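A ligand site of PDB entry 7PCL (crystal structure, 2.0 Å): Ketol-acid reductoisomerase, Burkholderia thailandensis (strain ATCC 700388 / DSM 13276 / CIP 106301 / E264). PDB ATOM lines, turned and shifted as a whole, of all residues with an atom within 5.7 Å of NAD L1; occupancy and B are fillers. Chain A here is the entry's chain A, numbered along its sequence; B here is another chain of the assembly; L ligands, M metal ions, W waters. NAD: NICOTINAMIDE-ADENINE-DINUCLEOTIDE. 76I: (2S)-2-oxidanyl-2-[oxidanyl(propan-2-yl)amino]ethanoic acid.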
ATOM      1  N   GLY A  30      29.167   8.153 -19.474  1.00  0.00           N
ATOM      2  CA  GLY A  30      28.051   9.031 -19.089  1.00  0.00           C
ATOM      3  C   GLY A  30      28.536  10.141 -18.167  1.00  0.00           C
ATOM      4  O   GLY A  30      29.543   9.926 -17.445  1.00  0.00           O
ATOM      5  N   TYR A  31      27.869  11.290 -18.211  1.00  0.00           N
ATOM      6  CA  TYR A  31      28.207  12.480 -17.384  1.00  0.00           C
ATOM      7  C   TYR A  31      26.900  13.112 -16.881  1.00  0.00           C
ATOM      8  O   TYR A  31      26.835  14.346 -16.728  1.00  0.00           O
ATOM      9  CB  TYR A  31      29.083  13.422 -18.203  1.00  0.00           C
ATOM     10  CG  TYR A  31      29.848  14.428 -17.376  1.00  0.00           C
ATOM     11  CD1 TYR A  31      30.993  14.056 -16.679  1.00  0.00           C
ATOM     12  CD2 TYR A  31      29.438  15.748 -17.291  1.00  0.00           C
ATOM     13  CE1 TYR A  31      31.704  14.972 -15.927  1.00  0.00           C
ATOM     14  CE2 TYR A  31      30.133  16.670 -16.536  1.00  0.00           C
ATOM     15  CZ  TYR A  31      31.273  16.289 -15.849  1.00  0.00           C
ATOM     16  OH  TYR A  31      31.955  17.198 -15.105  1.00  0.00           O
ATOM     17  N   GLY A  32      25.906  12.264 -16.596  1.00  0.00           N
ATOM     18  CA  GLY A  32      24.592  12.681 -16.080  1.00  0.00           C
ATOM     19  C   GLY A  32      24.618  12.854 -14.574  1.00  0.00           C
ATOM     20  O   GLY A  32      25.648  13.291 -14.041  1.00  0.00           O
ATOM     21  N   ILE A  33      23.509  12.492 -13.907  1.00  0.00           N
ATOM     22  CA  ILE A  33      23.292  12.717 -12.453  1.00  0.00           C
ATOM     23  C   ILE A  33      24.406  12.004 -11.669  1.00  0.00           C
ATOM     24  O   ILE A  33      25.054  12.670 -10.843  1.00  0.00           O
ATOM     25  CB  ILE A  33      21.883  12.234 -12.030  1.00  0.00           C
ATOM     26  CG1 ILE A  33      20.776  13.000 -12.753  1.00  0.00           C
ATOM     27  CG2 ILE A  33      21.719  12.313 -10.523  1.00  0.00           C
ATOM     28  CD1 ILE A  33      19.475  12.241 -12.874  1.00  0.00           C
ATOM     29  N   GLN A  34      24.638  10.720 -11.957  1.00  0.00           N
ATOM     30  CA  GLN A  34      25.670   9.895 -11.283  1.00  0.00           C
ATOM     31  C   GLN A  34      27.043  10.155 -11.916  1.00  0.00           C
ATOM     32  O   GLN A  34      27.992  10.433 -11.158  1.00  0.00           O
ATOM     33  CB  GLN A  34      25.300   8.409 -11.338  1.00  0.00           C
ATOM     34  CG  GLN A  34      24.140   8.045 -10.428  1.00  0.00           C
ATOM     35  CD  GLN A  34      24.453   8.300  -8.974  1.00  0.00           C
ATOM     36  OE1 GLN A  34      25.566   8.040  -8.514  1.00  0.00           O
ATOM     37  NE2 GLN A  34      23.477   8.802  -8.244  1.00  0.00           N
ATOM     38  N   GLY A  35      27.129  10.093 -13.255  1.00  0.00           N
ATOM     39  CA  GLY A  35      28.375  10.222 -14.030  1.00  0.00           C
ATOM     40  C   GLY A  35      29.199  11.436 -13.626  1.00  0.00           C
ATOM     41  O   GLY A  35      30.419  11.282 -13.439  1.00  0.00           O
ATOM     42  N   ASN A  53      31.414   9.691 -23.687  1.00  0.00           N
ATOM     43  CA  ASN A  53      30.038  10.239 -23.868  1.00  0.00           C
ATOM     44  C   ASN A  53      29.707  10.318 -25.356  1.00  0.00           C
ATOM     45  O   ASN A  53      30.623  10.560 -26.170  1.00  0.00           O
ATOM     46  CB  ASN A  53      29.884  11.586 -23.156  1.00  0.00           C
ATOM     47  CG  ASN A  53      28.455  11.885 -22.750  1.00  0.00           C
ATOM     48  OD1 ASN A  53      28.084  11.698 -21.600  1.00  0.00           O
ATOM     49  ND2 ASN A  53      27.658  12.356 -23.699  1.00  0.00           N
ATOM     50  N   ILE A  54      28.435  10.129 -25.677  1.00  0.00           N
ATOM     51  CA  ILE A  54      27.844  10.347 -27.030  1.00  0.00           C
ATOM     52  C   ILE A  54      27.831  11.859 -27.306  1.00  0.00           C
ATOM     53  O   ILE A  54      28.153  12.627 -26.389  1.00  0.00           O
ATOM     54  CB  ILE A  54      26.441   9.725 -27.128  1.00  0.00           C
ATOM     55  CG1 ILE A  54      25.456  10.343 -26.129  1.00  0.00           C
ATOM     56  CG2 ILE A  54      26.530   8.211 -26.971  1.00  0.00           C
ATOM     57  CD1 ILE A  54      24.010  10.071 -26.447  1.00  0.00           C
ATOM     58  N   ASP A  56      26.191  14.823 -27.289  1.00  0.00           N
ATOM     59  CA  ASP A  56      25.038  15.555 -26.701  1.00  0.00           C
ATOM     60  C   ASP A  56      25.584  16.615 -25.726  1.00  0.00           C
ATOM     61  O   ASP A  56      26.819  16.780 -25.670  1.00  0.00           O
ATOM     62  CB  ASP A  56      24.036  14.582 -26.075  1.00  0.00           C
ATOM     63  CG  ASP A  56      24.556  13.791 -24.876  1.00  0.00           C
ATOM     64  OD1 ASP A  56      25.627  14.164 -24.337  1.00  0.00           O
ATOM     65  OD2 ASP A  56      23.886  12.828 -24.484  1.00  0.00           O
ATOM     66  N   TYR A  58      25.918  16.736 -22.581  1.00  0.00           N
ATOM     67  CA  TYR A  58      26.709  16.152 -21.466  1.00  0.00           C
ATOM     68  C   TYR A  58      28.195  16.081 -21.872  1.00  0.00           C
ATOM     69  O   TYR A  58      29.064  16.279 -20.999  1.00  0.00           O
ATOM     70  CB  TYR A  58      26.154  14.781 -21.065  1.00  0.00           C
ATOM     71  CG  TYR A  58      24.738  14.777 -20.548  1.00  0.00           C
ATOM     72  CD1 TYR A  58      23.655  14.534 -21.379  1.00  0.00           C
ATOM     73  CD2 TYR A  58      24.471  14.952 -19.195  1.00  0.00           C
ATOM     74  CE1 TYR A  58      22.359  14.500 -20.897  1.00  0.00           C
ATOM     75  CE2 TYR A  58      23.184  14.919 -18.698  1.00  0.00           C
ATOM     76  CZ  TYR A  58      22.119  14.687 -19.550  1.00  0.00           C
ATOM     77  OH  TYR A  58      20.852  14.661 -19.060  1.00  0.00           O
ATOM     78  N   ILE A  72      32.525   6.810 -26.387  1.00  0.00           N
ATOM     79  CA  ILE A  72      32.526   5.756 -25.330  1.00  0.00           C
ATOM     80  C   ILE A  72      33.618   4.715 -25.639  1.00  0.00           C
ATOM     81  O   ILE A  72      34.383   4.393 -24.714  1.00  0.00           O
ATOM     82  CB  ILE A  72      31.118   5.135 -25.181  1.00  0.00           C
ATOM     83  CG1 ILE A  72      30.131   6.173 -24.630  1.00  0.00           C
ATOM     84  CG2 ILE A  72      31.156   3.873 -24.336  1.00  0.00           C
ATOM     85  CD1 ILE A  72      28.677   5.757 -24.702  1.00  0.00           C
ATOM     86  N   LEU A  84      29.758   2.314 -16.012  1.00  0.00           N
ATOM     87  CA  LEU A  84      28.656   2.501 -16.995  1.00  0.00           C
ATOM     88  C   LEU A  84      27.511   3.261 -16.325  1.00  0.00           C
ATOM     89  O   LEU A  84      26.603   2.605 -15.776  1.00  0.00           O
ATOM     90  CB  LEU A  84      28.200   1.126 -17.520  1.00  0.00           C
ATOM     91  CG  LEU A  84      27.082   1.159 -18.551  1.00  0.00           C
ATOM     92  CD1 LEU A  84      27.415   2.099 -19.703  1.00  0.00           C
ATOM     93  CD2 LEU A  84      26.797  -0.241 -19.085  1.00  0.00           C
ATOM     94  N   LEU A  85      27.582   4.597 -16.366  1.00  0.00           N
ATOM     95  CA  LEU A  85      26.634   5.514 -15.685  1.00  0.00           C
ATOM     96  C   LEU A  85      25.807   6.255 -16.739  1.00  0.00           C
ATOM     97  O   LEU A  85      25.868   7.495 -16.781  1.00  0.00           O
ATOM     98  CB  LEU A  85      27.423   6.446 -14.764  1.00  0.00           C
ATOM     99  CG  LEU A  85      28.291   5.735 -13.719  1.00  0.00           C
ATOM    100  CD1 LEU A  85      29.111   6.733 -12.914  1.00  0.00           C
ATOM    101  CD2 LEU A  85      27.431   4.896 -12.787  1.00  0.00           C
ATOM    102  N   ILE A  86      25.080   5.486 -17.554  1.00  0.00           N
ATOM    103  CA  ILE A  86      24.063   5.971 -18.532  1.00  0.00           C
ATOM    104  C   ILE A  86      22.745   5.284 -18.188  1.00  0.00           C
ATOM    105  O   ILE A  86      22.733   4.323 -17.422  1.00  0.00           O
ATOM    106  CB  ILE A  86      24.517   5.690 -19.979  1.00  0.00           C
ATOM    107  CG1 ILE A  86      24.545   4.186 -20.290  1.00  0.00           C
ATOM    108  CG2 ILE A  86      25.852   6.357 -20.263  1.00  0.00           C
ATOM    109  CD1 ILE A  86      24.943   3.855 -21.704  1.00  0.00           C
ATOM    110  N   PRO A  87      21.593   5.750 -18.721  1.00  0.00           N
ATOM    111  CA  PRO A  87      20.303   5.123 -18.435  1.00  0.00           C
ATOM    112  C   PRO A  87      20.276   3.611 -18.729  1.00  0.00           C
ATOM    113  O   PRO A  87      20.825   3.193 -19.737  1.00  0.00           O
ATOM    114  CB  PRO A  87      19.333   5.877 -19.353  1.00  0.00           C
ATOM    115  CG  PRO A  87      19.976   7.235 -19.513  1.00  0.00           C
ATOM    116  CD  PRO A  87      21.457   6.940 -19.573  1.00  0.00           C
ATOM    117  N   ASP A  88      19.621   2.853 -17.856  1.00  0.00           N
ATOM    118  CA  ASP A  88      19.687   1.370 -17.776  1.00  0.00           C
ATOM    119  C   ASP A  88      19.264   0.721 -19.093  1.00  0.00           C
ATOM    120  O   ASP A  88      19.898  -0.278 -19.482  1.00  0.00           O
ATOM    121  CB  ASP A  88      18.874   0.862 -16.594  1.00  0.00           C
ATOM    122  CG  ASP A  88      19.392   1.439 -15.293  1.00  0.00           C
ATOM    123  OD1 ASP A  88      20.428   0.941 -14.813  1.00  0.00           O
ATOM    124  OD2 ASP A  88      18.781   2.401 -14.791  1.00  0.00           O
ATOM    125  N   ALA A  90      19.747   1.679 -22.055  1.00  0.00           N
ATOM    126  CA  ALA A  90      20.795   1.921 -23.083  1.00  0.00           C
ATOM    127  C   ALA A  90      22.023   1.036 -22.847  1.00  0.00           C
ATOM    128  O   ALA A  90      22.959   1.100 -23.676  1.00  0.00           O
ATOM    129  CB  ALA A  90      21.173   3.384 -23.073  1.00  0.00           C
ATOM    130  N   HIS A  91      22.047   0.241 -21.770  1.00  0.00           N
ATOM    131  CA  HIS A  91      23.202  -0.602 -21.350  1.00  0.00           C
ATOM    132  C   HIS A  91      23.485  -1.677 -22.403  1.00  0.00           C
ATOM    133  O   HIS A  91      24.661  -1.828 -22.778  1.00  0.00           O
ATOM    134  CB  HIS A  91      22.947  -1.218 -19.968  1.00  0.00           C
ATOM    135  CG  HIS A  91      23.149  -0.262 -18.839  1.00  0.00           C
ATOM    136  ND1 HIS A  91      23.486  -0.686 -17.566  1.00  0.00           N
ATOM    137  CD2 HIS A  91      23.072   1.083 -18.790  1.00  0.00           C
ATOM    138  CE1 HIS A  91      23.596   0.364 -16.779  1.00  0.00           C
ATOM    139  NE2 HIS A  91      23.348   1.464 -17.501  1.00  0.00           N
ATOM    140  N   VAL A  94      25.102  -0.247 -25.828  1.00  0.00           N
ATOM    141  CA  VAL A  94      26.420   0.373 -25.500  1.00  0.00           C
ATOM    142  C   VAL A  94      27.409  -0.745 -25.101  1.00  0.00           C
ATOM    143  O   VAL A  94      28.564  -0.699 -25.560  1.00  0.00           O
ATOM    144  CB  VAL A  94      26.292   1.463 -24.418  1.00  0.00           C
ATOM    145  CG1 VAL A  94      27.646   1.919 -23.900  1.00  0.00           C
ATOM    146  CG2 VAL A  94      25.500   2.650 -24.931  1.00  0.00           C
ATOM    147  N   ALA A 112      25.777   0.896 -11.684  1.00  0.00           N
ATOM    148  CA  ALA A 112      25.281   1.565 -10.459  1.00  0.00           C
ATOM    149  C   ALA A 112      23.837   1.141 -10.162  1.00  0.00           C
ATOM    150  O   ALA A 112      23.195   1.789  -9.310  1.00  0.00           O
ATOM    151  CB  ALA A 112      25.416   3.062 -10.596  1.00  0.00           C
ATOM    152  N   HIS A 113      23.362   0.080 -10.816  1.00  0.00           N
ATOM    153  CA  HIS A 113      21.984  -0.470 -10.707  1.00  0.00           C
ATOM    154  C   HIS A 113      21.993  -1.869 -11.325  1.00  0.00           C
ATOM    155  O   HIS A 113      22.673  -2.057 -12.354  1.00  0.00           O
ATOM    156  CB  HIS A 113      20.994   0.510 -11.358  1.00  0.00           C
ATOM    157  CG  HIS A 113      19.549   0.153 -11.211  1.00  0.00           C
ATOM    158  ND1 HIS A 113      19.021  -0.371 -10.043  1.00  0.00           N
ATOM    159  CD2 HIS A 113      18.512   0.272 -12.065  1.00  0.00           C
ATOM    160  CE1 HIS A 113      17.731  -0.562 -10.200  1.00  0.00           C
ATOM    161  NE2 HIS A 113      17.390  -0.178 -11.425  1.00  0.00           N
ATOM    162  N   ALA A 134      26.228   0.563  -6.325  1.00  0.00           N
ATOM    163  CA  ALA A 134      24.937   1.267  -6.457  1.00  0.00           C
ATOM    164  C   ALA A 134      24.781   2.255  -5.301  1.00  0.00           C
ATOM    165  O   ALA A 134      24.467   1.835  -4.186  1.00  0.00           O
ATOM    166  CB  ALA A 134      23.819   0.260  -6.494  1.00  0.00           C
ATOM    167  N   PRO A 135      24.995   3.568  -5.519  1.00  0.00           N
ATOM    168  CA  PRO A 135      24.780   4.576  -4.471  1.00  0.00           C
ATOM    169  C   PRO A 135      23.299   4.677  -4.063  1.00  0.00           C
ATOM    170  O   PRO A 135      22.443   4.493  -4.926  1.00  0.00           O
ATOM    171  CB  PRO A 135      25.244   5.890  -5.120  1.00  0.00           C
ATOM    172  CG  PRO A 135      26.102   5.468  -6.298  1.00  0.00           C
ATOM    173  CD  PRO A 135      25.480   4.174  -6.768  1.00  0.00           C
ATOM    174  N   MET A 137      21.678   7.379  -3.178  1.00  0.00           N
ATOM    175  CA  MET A 137      21.603   8.862  -3.182  1.00  0.00           C
ATOM    176  C   MET A 137      21.856   9.360  -4.610  1.00  0.00           C
ATOM    177  O   MET A 137      22.598   8.683  -5.345  1.00  0.00           O
ATOM    178  CB  MET A 137      22.673   9.444  -2.249  1.00  0.00           C
ATOM    179  CG  MET A 137      22.563  10.941  -2.022  1.00  0.00           C
ATOM    180  SD  MET A 137      20.978  11.469  -1.320  1.00  0.00           S
ATOM    181  CE  MET A 137      20.947  10.532   0.201  1.00  0.00           C
ATOM    182  N   TYR A 138      21.287  10.523  -4.963  1.00  0.00           N
ATOM    183  CA  TYR A 138      21.488  11.175  -6.277  1.00  0.00           C
ATOM    184  C   TYR A 138      22.762  12.043  -6.209  1.00  0.00           C
ATOM    185  O   TYR A 138      23.373  12.140  -5.129  1.00  0.00           O
ATOM    186  CB  TYR A 138      20.222  11.904  -6.761  1.00  0.00           C
ATOM    187  CG  TYR A 138      19.486  12.786  -5.774  1.00  0.00           C
ATOM    188  CD1 TYR A 138      19.697  14.150  -5.730  1.00  0.00           C
ATOM    189  CD2 TYR A 138      18.504  12.253  -4.949  1.00  0.00           C
ATOM    190  CE1 TYR A 138      18.994  14.966  -4.864  1.00  0.00           C
ATOM    191  CE2 TYR A 138      17.785  13.054  -4.072  1.00  0.00           C
ATOM    192  CZ  TYR A 138      18.033  14.415  -4.025  1.00  0.00           C
ATOM    193  OH  TYR A 138      17.332  15.211  -3.173  1.00  0.00           O
ATOM    194  N   GLY A 139      23.157  12.605  -7.360  1.00  0.00           N
ATOM    195  CA  GLY A 139      24.511  13.126  -7.626  1.00  0.00           C
ATOM    196  C   GLY A 139      24.878  14.344  -6.800  1.00  0.00           C
ATOM    197  O   GLY A 139      25.997  14.356  -6.239  1.00  0.00           O
ATOM    198  N   ASP A 196      15.423  -0.997  -5.250  1.00  0.00           N
ATOM    199  CA  ASP A 196      15.599   0.337  -5.875  1.00  0.00           C
ATOM    200  C   ASP A 196      14.320   0.707  -6.643  1.00  0.00           C
ATOM    201  O   ASP A 196      13.805   1.810  -6.410  1.00  0.00           O
ATOM    202  CB  ASP A 196      16.826   0.351  -6.783  1.00  0.00           C
ATOM    203  CG  ASP A 196      17.296   1.754  -7.136  1.00  0.00           C
ATOM    204  OD1 ASP A 196      17.832   2.430  -6.230  1.00  0.00           O
ATOM    205  OD2 ASP A 196      17.104   2.155  -8.302  1.00  0.00           O
ATOM    206  N   GLU B 237      17.666   9.646   1.517  1.00  0.00           N
ATOM    207  CA  GLU B 237      17.338   9.950   0.101  1.00  0.00           C
ATOM    208  C   GLU B 237      15.912  10.505   0.001  1.00  0.00           C
ATOM    209  O   GLU B 237      15.738  11.536  -0.668  1.00  0.00           O
ATOM    210  CB  GLU B 237      17.501   8.717  -0.799  1.00  0.00           C
ATOM    211  CG  GLU B 237      17.505   9.072  -2.272  1.00  0.00           C
ATOM    212  CD  GLU B 237      17.846   7.940  -3.214  1.00  0.00           C
ATOM    213  OE1 GLU B 237      17.526   6.774  -2.888  1.00  0.00           O
ATOM    214  OE2 GLU B 237      18.433   8.222  -4.278  1.00  0.00           O
ATOM    215  N   GLN B 257      16.505  14.808 -10.908  1.00  0.00           N
ATOM    216  CA  GLN B 257      17.508  13.992 -10.147  1.00  0.00           C
ATOM    217  C   GLN B 257      17.316  12.483 -10.366  1.00  0.00           C
ATOM    218  O   GLN B 257      18.214  11.726  -9.948  1.00  0.00           O
ATOM    219  CB  GLN B 257      17.408  14.292  -8.657  1.00  0.00           C
ATOM    220  CG  GLN B 257      17.633  15.761  -8.297  1.00  0.00           C
ATOM    221  CD  GLN B 257      19.074  16.185  -8.460  1.00  0.00           C
ATOM    222  OE1 GLN B 257      19.871  15.543  -9.144  1.00  0.00           O
ATOM    223  NE2 GLN B 257      19.431  17.282  -7.806  1.00  0.00           N
ATOM    224  N   GLY B 258      16.206  12.053 -10.964  1.00  0.00           N
ATOM    225  CA  GLY B 258      15.915  10.624 -11.193  1.00  0.00           C
ATOM    226  C   GLY B 258      16.428  10.155 -12.535  1.00  0.00           C
ATOM    227  O   GLY B 258      16.256  10.905 -13.524  1.00  0.00           O
ATOM    228  N   SER B 259      17.040   8.963 -12.597  1.00  0.00           N
ATOM    229  CA  SER B 259      17.351   8.256 -13.862  1.00  0.00           C
ATOM    230  C   SER B 259      16.059   8.109 -14.660  1.00  0.00           C
ATOM    231  O   SER B 259      14.964   8.194 -14.105  1.00  0.00           O
ATOM    232  CB  SER B 259      17.989   6.908 -13.604  1.00  0.00           C
ATOM    233  OG  SER B 259      17.023   5.953 -13.176  1.00  0.00           O
ATOM    234  N   PRO B 260      16.122   7.900 -16.006  1.00  0.00           N
ATOM    235  CA  PRO B 260      14.916   7.654 -16.791  1.00  0.00           C
ATOM    236  C   PRO B 260      14.146   6.429 -16.265  1.00  0.00           C
ATOM    237  O   PRO B 260      12.929   6.467 -16.258  1.00  0.00           O
ATOM    238  CB  PRO B 260      15.459   7.451 -18.214  1.00  0.00           C
ATOM    239  CG  PRO B 260      16.767   8.218 -18.195  1.00  0.00           C
ATOM    240  CD  PRO B 260      17.336   7.902 -16.834  1.00  0.00           C
ATOM    241  N   THR B 261      14.868   5.386 -15.834  1.00  0.00           N
ATOM    242  CA  THR B 261      14.308   4.180 -15.172  1.00  0.00           C
ATOM    243  C   THR B 261      13.425   4.607 -14.005  1.00  0.00           C
ATOM    244  O   THR B 261      12.273   4.137 -13.912  1.00  0.00           O
ATOM    245  CB  THR B 261      15.420   3.243 -14.675  1.00  0.00           C
ATOM    246  OG1 THR B 261      16.314   3.010 -15.766  1.00  0.00           O
ATOM    247  CG2 THR B 261      14.894   1.918 -14.157  1.00  0.00           C
HETATM  248  PA  NAD L   1      21.002  10.269 -16.661  1.00  0.00           P
HETATM  249  O1A NAD L   1      19.654  10.270 -17.265  1.00  0.00           O
HETATM  250  O2A NAD L   1      21.428  11.465 -15.907  1.00  0.00           O
HETATM  251  O5B NAD L   1      22.097   9.909 -17.766  1.00  0.00           O
HETATM  252  C5B NAD L   1      22.495  10.884 -18.748  1.00  0.00           C
HETATM  253  C4B NAD L   1      23.803  10.440 -19.369  1.00  0.00           C
HETATM  254  O4B NAD L   1      23.607   9.220 -20.121  1.00  0.00           O
HETATM  255  C3B NAD L   1      24.457  11.440 -20.337  1.00  0.00           C
HETATM  256  O3B NAD L   1      25.867  11.390 -20.201  1.00  0.00           O
HETATM  257  C2B NAD L   1      23.999  10.911 -21.702  1.00  0.00           C
HETATM  258  O2B NAD L   1      24.871  11.247 -22.751  1.00  0.00           O
HETATM  259  C1B NAD L   1      24.010   9.408 -21.452  1.00  0.00           C
HETATM  260  N9A NAD L   1      23.137   8.661 -22.352  1.00  0.00           N
HETATM  261  C8A NAD L   1      21.778   8.771 -22.435  1.00  0.00           C
HETATM  262  N7A NAD L   1      21.251   7.985 -23.340  1.00  0.00           N
HETATM  263  C5A NAD L   1      22.340   7.309 -23.882  1.00  0.00           C
HETATM  264  C6A NAD L   1      22.433   6.336 -24.886  1.00  0.00           C
HETATM  265  N6A NAD L   1      21.389   5.851 -25.553  1.00  0.00           N
HETATM  266  N1A NAD L   1      23.667   5.874 -25.187  1.00  0.00           N
HETATM  267  C2A NAD L   1      24.715   6.371 -24.524  1.00  0.00           C
HETATM  268  N3A NAD L   1      24.737   7.284 -23.557  1.00  0.00           N
HETATM  269  C4A NAD L   1      23.503   7.730 -23.284  1.00  0.00           C
HETATM  270  O3  NAD L   1      21.171   8.963 -15.774  1.00  0.00           O
HETATM  271  PN  NAD L   1      21.542   8.667 -14.255  1.00  0.00           P
HETATM  272  O1N NAD L   1      20.376   9.036 -13.417  1.00  0.00           O
HETATM  273  O2N NAD L   1      22.860   9.293 -13.962  1.00  0.00           O
HETATM  274  O5D NAD L   1      21.712   7.091 -14.259  1.00  0.00           O
HETATM  275  C5D NAD L   1      22.966   6.480 -14.631  1.00  0.00           C
HETATM  276  C4D NAD L   1      23.053   5.107 -13.996  1.00  0.00           C
HETATM  277  O4D NAD L   1      23.157   5.282 -12.565  1.00  0.00           O
HETATM  278  C3D NAD L   1      21.836   4.198 -14.232  1.00  0.00           C
HETATM  279  O3D NAD L   1      22.246   2.855 -14.399  1.00  0.00           O
HETATM  280  C2D NAD L   1      21.008   4.445 -12.964  1.00  0.00           C
HETATM  281  O2D NAD L   1      20.134   3.371 -12.671  1.00  0.00           O
HETATM  282  C1D NAD L   1      22.110   4.582 -11.914  1.00  0.00           C
HETATM  283  N1N NAD L   1      21.692   5.337 -10.706  1.00  0.00           N
HETATM  284  C2N NAD L   1      21.107   6.574 -10.811  1.00  0.00           C
HETATM  285  C3N NAD L   1      20.847   7.316  -9.665  1.00  0.00           C
HETATM  286  C7N NAD L   1      20.371   8.739  -9.780  1.00  0.00           C
HETATM  287  O7N NAD L   1      20.362   9.452  -8.792  1.00  0.00           O
HETATM  288  N7N NAD L   1      20.005   9.177 -10.979  1.00  0.00           N
HETATM  289  C4N NAD L   1      21.083   6.739  -8.425  1.00  0.00           C
HETATM  290  C5N NAD L   1      21.761   5.549  -8.350  1.00  0.00           C
HETATM  291  C6N NAD L   1      21.907   4.798  -9.489  1.00  0.00           C
HETATM  292  C8  76I L   2      16.677   7.945  -7.460  1.00  0.00           C
HETATM  293  C10 76I L   2      15.582   7.737  -6.417  1.00  0.00           C
HETATM  294  O3  76I L   2      17.326   7.622 -10.055  1.00  0.00           O
HETATM  295  C1  76I L   2      17.462   6.433  -9.724  1.00  0.00           C
HETATM  296  O2  76I L   2      17.166   5.457 -10.449  1.00  0.00           O
HETATM  297  C3  76I L   2      18.144   6.108  -8.376  1.00  0.00           C
HETATM  298  O6  76I L   2      17.898   4.763  -8.009  1.00  0.00           O
HETATM  299  N5  76I L   2      17.840   7.056  -7.257  1.00  0.00           N
HETATM  300  O7  76I L   2      17.769   6.343  -5.907  1.00  0.00           O
HETATM  301  C9  76I L   2      17.133   9.407  -7.399  1.00  0.00           C
HETATM  302 MG    MG M   1      17.269   3.558  -9.627  1.00  0.00          MG
HETATM  303 MG    MG M   2      18.065   4.444  -5.943  1.00  0.00          MG
HETATM  304  O   HOH W   1      20.800  14.000 -16.510  1.00  0.00           O
HETATM  305  O   HOH W   2      20.692   2.056  -8.194  1.00  0.00           O
HETATM  306  O   HOH W   3      20.103   3.864  -6.053  1.00  0.00           O
HETATM  307  O   HOH W   4      18.567   7.227 -22.945  1.00  0.00           O
HETATM  308  O   HOH W   5      26.953   8.976 -23.308  1.00  0.00           O
HETATM  309  O   HOH W   6      25.156   9.635 -15.403  1.00  0.00           O
HETATM  310  O   HOH W   7      24.751   1.719 -14.042  1.00  0.00           O
HETATM  311  O   HOH W   8      17.271  11.450 -16.143  1.00  0.00           O
HETATM  312  O   HOH W   9      19.204   3.122 -10.159  1.00  0.00           O
HETATM  313  O   HOH W  10      19.268  10.597 -19.957  1.00  0.00           O
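Water W1 lies within hydrogen-bond range of the side-chain hydroxyl of Tyr 58 (2.6 Å) and an oxygen (O2A) of NAD L1 (2.7 Å).
Water W6 lies within hydrogen-bond range of the backbone carbonyl oxygen of Leu 85 (2.6 Å), an oxygen (O2N) of NAD L1 (2.7 Å), the backbone NH of Gly 35 (3.0 Å) and the backbone NH of Gly 32 (3.0 Å).
Water W7 lies within hydrogen-bond range of the backbone carbonyl oxygen of Leu 84, the backbone NH of Ala 112 and an oxygen (O3D) of NAD L1.
Water W5 lies within hydrogen-bond range of N3A of NAD L1 (2.8 Å), N of Ile 54 (3.0 Å) and OD1 of Asn 53 (3.4 Å).
Water W8 bridges O of Gly 258 of chain B (2.9 Å) and O1A of NAD L1 (2.9 Å).
Water W2 lies within hydrogen-bond range of O of Ala 112 and ND1 of His 113.
Merely in contact with NAD L1: Gly 30 (3.4 Å), Gly 32 (3.4 Å), Ile 54 (3.5 Å), Tyr 58 (3.4 Å), Leu 85 (3.5 Å), Pro 87 (3.2 Å), Ala 90 (3.5 Å), His 91 (3.6 Å), Val 94 (3.7 Å), Ala 112 (3.3 Å), His 113 (3.3 Å), Pro 135 (3.6 Å), Met 137 (3.9 Å), Tyr 138 (3.2 Å) and Pro 260 of chain B (3.3 Å).
Hydrophobic or aromatic side chains that line NAD L1: Ile 33, Ile 54, Tyr 58, Ile 86, Pro 87, Ala 90, His 91, Val 94, Ala 112, His 113, Tyr 138 and Pro 260 of chain B.
Within 4 Å of NAD L1: Gly 30, Tyr 31, Gly 32, Ile 33, Gln 34, Asn 53, Ile 54, Asp 56, Tyr 58, Leu 85, Ile 86, Pro 87, Asp 88, Ala 90, His 91, Val 94, Ala 112, His 113, Pro 135, Met 137, Tyr 138, Gln 257 of chain B, Ser 259 of chain B and Pro 260 of chain B.
The nearest printed residue that does not touch NAD L1 is Ile 72 (4.01 Å).
An oxygen (O3) of 76I L2 lies within hydrogen-bond range of a nitrogen (N7N) of NAD L1 (3.2 Å).
The side-chain carboxylate of Asp 56 is in hydrogen-bond range of the side-chain amide nitrogen of Asn 53 (2.8 Å).
The side-chain carboxylate of Asp 56 sits at hydrogen-bond distance from the backbone NH of Tyr 58, at 3.1 Å.
OD1 of Asn 53 lies within hydrogen-bond range of N of Tyr 31.
The side-chain carboxylate of Asp 88 sits at hydrogen-bond distance from the side-chain hydroxyl of Thr 261 of chain B.
The backbone carbonyl oxygen of Met 137 sits at hydrogen-bond distance from the side-chain amide nitrogen of Gln 34 (3.0 Å).
OG of Ser 259 of chain B lies close to N of Thr 261 of chain B.
The backbone carbonyl oxygen of Ile 86 is in hydrogen-bond range of a ring nitrogen (NE2) of His 91 (2.9 Å).
An oxygen (O2B) of NAD L1 is in hydrogen-bond range of the side-chain carboxylate of Asp 56 (2.5 Å).
The side-chain amide oxygen (OD1) of Asn 53 lies within hydrogen-bond range of an oxygen (O3B) of NAD L1.
The side-chain carboxylate of Asp 88 sits at hydrogen-bond distance from an oxygen (O3D) of NAD L1, 2.7 Å away.
The backbone NH of Tyr 31 is in hydrogen-bond range of an oxygen (O3B) of NAD L1 (2.8 Å).
An oxygen (O2N) of NAD L1 is in hydrogen-bond range of the backbone NH of Gln 34 (3.0 Å).
An oxygen (O7N) of NAD L1 lies close to the side-chain amide nitrogen (NE2) of Gln 34 (3.2 Å).
An oxygen (O2A) of NAD L1 lies within hydrogen-bond range of the backbone NH (N) of Ile 33 (3.1 Å).
An oxygen (O1N) of NAD L1 sits close to the backbone NH of Ser 259 of chain B (3.4 Å).
The backbone carbonyl oxygen (O) of Gln 257 of chain B sits at hydrogen-bond distance from a nitrogen (N7N) of NAD L1 (3.3 Å).
An oxygen (O3D) of NAD L1 sits close to the backbone carbonyl oxygen (O) of Ile 86, 3.4 Å away.
N of Ser 259 of chain B is in hydrogen-bond range of O3 of 76I L2, 2.9 Å away.
An oxygen (O2) of 76I L2 lies close to the side-chain hydroxyl of Ser 259 of chain B (2.8 Å).
O7 of 76I L2 sits close to OE2 of Glu 237 of chain B (2.6 Å).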
